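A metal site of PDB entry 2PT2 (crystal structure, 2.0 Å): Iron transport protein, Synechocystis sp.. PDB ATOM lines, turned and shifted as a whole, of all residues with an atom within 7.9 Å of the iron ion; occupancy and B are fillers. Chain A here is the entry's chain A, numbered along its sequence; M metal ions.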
ATOM      1  N   SER A  26      -6.689  25.091  27.491  1.00  0.00           N
ATOM      2  CA  SER A  26      -7.713  24.764  26.532  1.00  0.00           C
ATOM      3  C   SER A  26      -8.251  23.355  26.811  1.00  0.00           C
ATOM      4  O   SER A  26      -9.067  22.833  26.047  1.00  0.00           O
ATOM      5  CB  SER A  26      -7.188  24.886  25.086  1.00  0.00           C
ATOM      6  OG  SER A  26      -5.978  24.179  24.871  1.00  0.00           O
ATOM      7  N   ARG A  27      -7.788  22.735  27.896  1.00  0.00           N
ATOM      8  CA  ARG A  27      -8.331  21.428  28.278  1.00  0.00           C
ATOM      9  C   ARG A  27      -9.727  21.802  28.745  1.00  0.00           C
ATOM     10  O   ARG A  27      -9.917  22.834  29.388  1.00  0.00           O
ATOM     11  CB  ARG A  27      -7.547  20.780  29.424  1.00  0.00           C
ATOM     12  CG  ARG A  27      -6.306  20.023  28.973  1.00  0.00           C
ATOM     13  CD  ARG A  27      -5.615  19.344  30.158  1.00  0.00           C
ATOM     14  NE  ARG A  27      -6.297  18.130  30.613  1.00  0.00           N
ATOM     15  CZ  ARG A  27      -6.235  16.952  30.002  1.00  0.00           C
ATOM     16  NH1 ARG A  27      -5.524  16.818  28.886  1.00  0.00           N
ATOM     17  NH2 ARG A  27      -6.848  15.906  30.516  1.00  0.00           N
ATOM     18  N   HIS A  28     -10.693  20.947  28.443  1.00  0.00           N
ATOM     19  CA  HIS A  28     -12.099  21.199  28.747  1.00  0.00           C
ATOM     20  C   HIS A  28     -12.794  20.006  29.406  1.00  0.00           C
ATOM     21  O   HIS A  28     -13.929  19.679  29.025  1.00  0.00           O
ATOM     22  CB  HIS A  28     -12.815  21.511  27.438  1.00  0.00           C
ATOM     23  CG  HIS A  28     -12.713  20.398  26.429  1.00  0.00           C
ATOM     24  ND1 HIS A  28     -13.737  19.511  26.205  1.00  0.00           N
ATOM     25  CD2 HIS A  28     -11.693  20.017  25.633  1.00  0.00           C
ATOM     26  CE1 HIS A  28     -13.356  18.620  25.303  1.00  0.00           C
ATOM     27  NE2 HIS A  28     -12.109  18.902  24.947  1.00  0.00           N
ATOM     28  N   TYR A  29     -12.148  19.366  30.370  1.00  0.00           N
ATOM     29  CA  TYR A  29     -12.720  18.189  31.007  1.00  0.00           C
ATOM     30  C   TYR A  29     -13.167  18.383  32.456  1.00  0.00           C
ATOM     31  O   TYR A  29     -12.586  19.183  33.190  1.00  0.00           O
ATOM     32  CB  TYR A  29     -11.716  17.038  30.920  1.00  0.00           C
ATOM     33  CG  TYR A  29     -11.165  16.890  29.513  1.00  0.00           C
ATOM     34  CD1 TYR A  29      -9.877  17.339  29.190  1.00  0.00           C
ATOM     35  CD2 TYR A  29     -11.962  16.365  28.498  1.00  0.00           C
ATOM     36  CE1 TYR A  29      -9.399  17.267  27.880  1.00  0.00           C
ATOM     37  CE2 TYR A  29     -11.493  16.288  27.185  1.00  0.00           C
ATOM     38  CZ  TYR A  29     -10.217  16.749  26.877  1.00  0.00           C
ATOM     39  OH  TYR A  29      -9.777  16.689  25.580  1.00  0.00           O
ATOM     40  N   VAL A  76      -4.598  21.017  23.962  1.00  0.00           N
ATOM     41  CA  VAL A  76      -5.026  19.647  23.700  1.00  0.00           C
ATOM     42  C   VAL A  76      -4.733  19.413  22.228  1.00  0.00           C
ATOM     43  O   VAL A  76      -5.473  18.719  21.532  1.00  0.00           O
ATOM     44  CB  VAL A  76      -6.534  19.433  23.962  1.00  0.00           C
ATOM     45  CG1 VAL A  76      -6.817  19.540  25.462  1.00  0.00           C
ATOM     46  CG2 VAL A  76      -7.365  20.457  23.187  1.00  0.00           C
ATOM     47  N   ARG A 119      -3.677  11.057  22.637  1.00  0.00           N
ATOM     48  CA  ARG A 119      -5.024  10.664  22.266  1.00  0.00           C
ATOM     49  C   ARG A 119      -5.015  10.361  20.769  1.00  0.00           C
ATOM     50  O   ARG A 119      -4.313  11.018  19.998  1.00  0.00           O
ATOM     51  CB  ARG A 119      -6.037  11.777  22.581  1.00  0.00           C
ATOM     52  CG  ARG A 119      -5.693  13.169  22.042  1.00  0.00           C
ATOM     53  CD  ARG A 119      -4.865  14.007  23.025  1.00  0.00           C
ATOM     54  NE  ARG A 119      -5.612  14.376  24.227  1.00  0.00           N
ATOM     55  CZ  ARG A 119      -6.653  15.218  24.252  1.00  0.00           C
ATOM     56  NH1 ARG A 119      -7.085  15.776  23.126  1.00  0.00           N
ATOM     57  NH2 ARG A 119      -7.250  15.506  25.396  1.00  0.00           N
ATOM     58  N   ARG A 121      -7.093   9.927  17.139  1.00  0.00           N
ATOM     59  CA  ARG A 121      -8.327  10.312  16.465  1.00  0.00           C
ATOM     60  C   ARG A 121      -8.597   9.116  15.560  1.00  0.00           C
ATOM     61  O   ARG A 121      -7.908   8.912  14.559  1.00  0.00           O
ATOM     62  CB  ARG A 121      -8.153  11.590  15.637  1.00  0.00           C
ATOM     63  CG  ARG A 121      -9.480  12.267  15.304  1.00  0.00           C
ATOM     64  CD  ARG A 121      -9.302  13.750  14.949  1.00  0.00           C
ATOM     65  NE  ARG A 121     -10.581  14.446  14.828  1.00  0.00           N
ATOM     66  CZ  ARG A 121     -11.438  14.615  15.833  1.00  0.00           C
ATOM     67  NH1 ARG A 121     -11.157  14.147  17.038  1.00  0.00           N
ATOM     68  NH2 ARG A 121     -12.571  15.267  15.633  1.00  0.00           N
ATOM     69  N   ARG A 153     -17.339  16.628  13.302  1.00  0.00           N
ATOM     70  CA  ARG A 153     -17.504  17.985  13.806  1.00  0.00           C
ATOM     71  C   ARG A 153     -16.880  18.999  12.841  1.00  0.00           C
ATOM     72  O   ARG A 153     -16.183  18.620  11.898  1.00  0.00           O
ATOM     73  CB  ARG A 153     -16.870  18.110  15.198  1.00  0.00           C
ATOM     74  CG  ARG A 153     -15.354  18.092  15.197  1.00  0.00           C
ATOM     75  CD  ARG A 153     -14.833  17.979  16.612  1.00  0.00           C
ATOM     76  NE  ARG A 153     -15.263  19.081  17.474  1.00  0.00           N
ATOM     77  CZ  ARG A 153     -15.057  19.102  18.789  1.00  0.00           C
ATOM     78  NH1 ARG A 153     -14.435  18.082  19.371  1.00  0.00           N
ATOM     79  NH2 ARG A 153     -15.453  20.129  19.523  1.00  0.00           N
ATOM     80  N   ASN A 157     -12.512  23.005  14.462  1.00  0.00           N
ATOM     81  CA  ASN A 157     -11.896  22.261  15.554  1.00  0.00           C
ATOM     82  C   ASN A 157     -10.454  21.853  15.262  1.00  0.00           C
ATOM     83  O   ASN A 157     -10.144  21.354  14.185  1.00  0.00           O
ATOM     84  CB  ASN A 157     -12.746  21.029  15.885  1.00  0.00           C
ATOM     85  CG  ASN A 157     -12.060  20.084  16.845  1.00  0.00           C
ATOM     86  OD1 ASN A 157     -11.472  19.078  16.438  1.00  0.00           O
ATOM     87  ND2 ASN A 157     -12.122  20.391  18.135  1.00  0.00           N
ATOM     88  N   TYR A 159      -8.629  19.398  16.481  1.00  0.00           N
ATOM     89  CA  TYR A 159      -8.377  17.969  16.349  1.00  0.00           C
ATOM     90  C   TYR A 159      -8.461  17.641  14.846  1.00  0.00           C
ATOM     91  O   TYR A 159      -7.639  16.894  14.324  1.00  0.00           O
ATOM     92  CB  TYR A 159      -9.442  17.155  17.096  1.00  0.00           C
ATOM     93  CG  TYR A 159      -9.532  17.429  18.592  1.00  0.00           C
ATOM     94  CD1 TYR A 159     -10.720  17.213  19.281  1.00  0.00           C
ATOM     95  CD2 TYR A 159      -8.419  17.845  19.318  1.00  0.00           C
ATOM     96  CE1 TYR A 159     -10.814  17.408  20.654  1.00  0.00           C
ATOM     97  CE2 TYR A 159      -8.493  18.043  20.701  1.00  0.00           C
ATOM     98  CZ  TYR A 159      -9.692  17.821  21.363  1.00  0.00           C
ATOM     99  OH  TYR A 159      -9.768  17.974  22.730  1.00  0.00           O
ATOM    100  N   ASP A 195     -17.152  15.911  19.448  1.00  0.00           N
ATOM    101  CA  ASP A 195     -16.872  14.497  19.179  1.00  0.00           C
ATOM    102  C   ASP A 195     -17.915  13.560  19.779  1.00  0.00           C
ATOM    103  O   ASP A 195     -18.331  12.594  19.134  1.00  0.00           O
ATOM    104  CB  ASP A 195     -15.491  14.102  19.712  1.00  0.00           C
ATOM    105  CG  ASP A 195     -14.361  14.439  18.758  1.00  0.00           C
ATOM    106  OD1 ASP A 195     -13.235  13.914  18.954  1.00  0.00           O
ATOM    107  OD2 ASP A 195     -14.570  15.238  17.821  1.00  0.00           O
ATOM    108  N   ASN A 213     -11.787  11.351  19.107  1.00  0.00           N
ATOM    109  CA  ASN A 213     -10.670  10.956  19.951  1.00  0.00           C
ATOM    110  C   ASN A 213     -11.082   9.806  20.853  1.00  0.00           C
ATOM    111  O   ASN A 213     -12.192   9.766  21.389  1.00  0.00           O
ATOM    112  CB  ASN A 213     -10.166  12.135  20.792  1.00  0.00           C
ATOM    113  CG  ASN A 213      -9.505  13.218  19.945  1.00  0.00           C
ATOM    114  OD1 ASN A 213      -9.068  12.969  18.828  1.00  0.00           O
ATOM    115  ND2 ASN A 213      -9.419  14.426  20.509  1.00  0.00           N
ATOM    116  N   TYR A 215     -10.413   8.843  23.940  1.00  0.00           N
ATOM    117  CA  TYR A 215     -10.876   9.089  25.304  1.00  0.00           C
ATOM    118  C   TYR A 215     -12.353   9.462  25.417  1.00  0.00           C
ATOM    119  O   TYR A 215     -12.939   9.339  26.484  1.00  0.00           O
ATOM    120  CB  TYR A 215      -9.972  10.134  25.982  1.00  0.00           C
ATOM    121  CG  TYR A 215      -9.962  11.481  25.310  1.00  0.00           C
ATOM    122  CD1 TYR A 215     -10.950  12.423  25.590  1.00  0.00           C
ATOM    123  CD2 TYR A 215      -8.984  11.810  24.373  1.00  0.00           C
ATOM    124  CE1 TYR A 215     -10.971  13.647  24.948  1.00  0.00           C
ATOM    125  CE2 TYR A 215      -8.996  13.030  23.714  1.00  0.00           C
ATOM    126  CZ  TYR A 215      -9.996  13.947  24.004  1.00  0.00           C
ATOM    127  OH  TYR A 215     -10.049  15.142  23.330  1.00  0.00           O
ATOM    128  N   TYR A 216     -12.970   9.889  24.314  1.00  0.00           N
ATOM    129  CA  TYR A 216     -14.396  10.222  24.358  1.00  0.00           C
ATOM    130  C   TYR A 216     -15.218   8.934  24.442  1.00  0.00           C
ATOM    131  O   TYR A 216     -16.258   8.895  25.092  1.00  0.00           O
ATOM    132  CB  TYR A 216     -14.839  11.013  23.116  1.00  0.00           C
ATOM    133  CG  TYR A 216     -14.352  12.442  23.112  1.00  0.00           C
ATOM    134  CD1 TYR A 216     -13.462  12.905  22.142  1.00  0.00           C
ATOM    135  CD2 TYR A 216     -14.731  13.325  24.130  1.00  0.00           C
ATOM    136  CE1 TYR A 216     -12.949  14.190  22.190  1.00  0.00           C
ATOM    137  CE2 TYR A 216     -14.227  14.620  24.183  1.00  0.00           C
ATOM    138  CZ  TYR A 216     -13.336  15.044  23.208  1.00  0.00           C
ATOM    139  OH  TYR A 216     -12.799  16.317  23.281  1.00  0.00           O
ATOM    140  N   ASN A 286      -9.442  10.241  32.921  1.00  0.00           N
ATOM    141  CA  ASN A 286      -9.808  10.998  31.735  1.00  0.00           C
ATOM    142  C   ASN A 286      -9.665  10.155  30.471  1.00  0.00           C
ATOM    143  O   ASN A 286      -9.862  10.634  29.361  1.00  0.00           O
ATOM    144  CB  ASN A 286      -8.992  12.278  31.582  1.00  0.00           C
ATOM    145  CG  ASN A 286      -9.748  13.323  30.771  1.00  0.00           C
ATOM    146  OD1 ASN A 286      -9.188  14.000  29.905  1.00  0.00           O
ATOM    147  ND2 ASN A 286     -11.040  13.454  31.052  1.00  0.00           N
ATOM    148  N   GLU A 288      -7.171   8.980  28.725  1.00  0.00           N
ATOM    149  CA  GLU A 288      -6.158   9.296  27.717  1.00  0.00           C
ATOM    150  C   GLU A 288      -4.995   8.317  27.845  1.00  0.00           C
ATOM    151  O   GLU A 288      -4.946   7.526  28.793  1.00  0.00           O
ATOM    152  CB  GLU A 288      -5.651  10.728  27.892  1.00  0.00           C
ATOM    153  CG  GLU A 288      -6.729  11.790  27.689  1.00  0.00           C
ATOM    154  CD  GLU A 288      -6.306  13.165  28.162  1.00  0.00           C
ATOM    155  OE1 GLU A 288      -5.671  13.906  27.387  1.00  0.00           O
ATOM    156  OE2 GLU A 288      -6.606  13.503  29.329  1.00  0.00           O
HETATM  157 FE    FE M   1     -10.935  16.879  23.919  1.00  0.00          FE
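The side-chain hydroxyl of Tyr 159 lies close to the guanidinium group of Arg 119 (3.5 Å). The backbone NH of Tyr 159 is in hydrogen-bond range of the side-chain amide oxygen of Asn 157 (2.9 Å). The guanidinium group (NH2) of Arg 119 sits close to the side-chain hydroxyl (OH) of Tyr 29 (2.8 Å). The guanidinium group of Arg 119 sits close to the side-chain hydroxyl of Tyr 215, at 3.0 Å. ND2 of Asn 213 sits close to OH of Tyr 215 (3.0 Å).
Along chain A the residues within 4 Å of the iron ion span positions 28 to 216. The nearest printed residue that does not touch the iron ion is Arg 119 (4.1 Å).
The iron ion is bound by the side-chain hydroxyl (OH) of Tyr 159, the side-chain hydroxyl (OH) of Tyr 29, the side-chain hydroxyl (OH) of Tyr 215, the side-chain hydroxyl (OH) of Tyr 216 and a ring nitrogen (NE2) of His 28. The iron ion has five donor atoms within binding distance.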
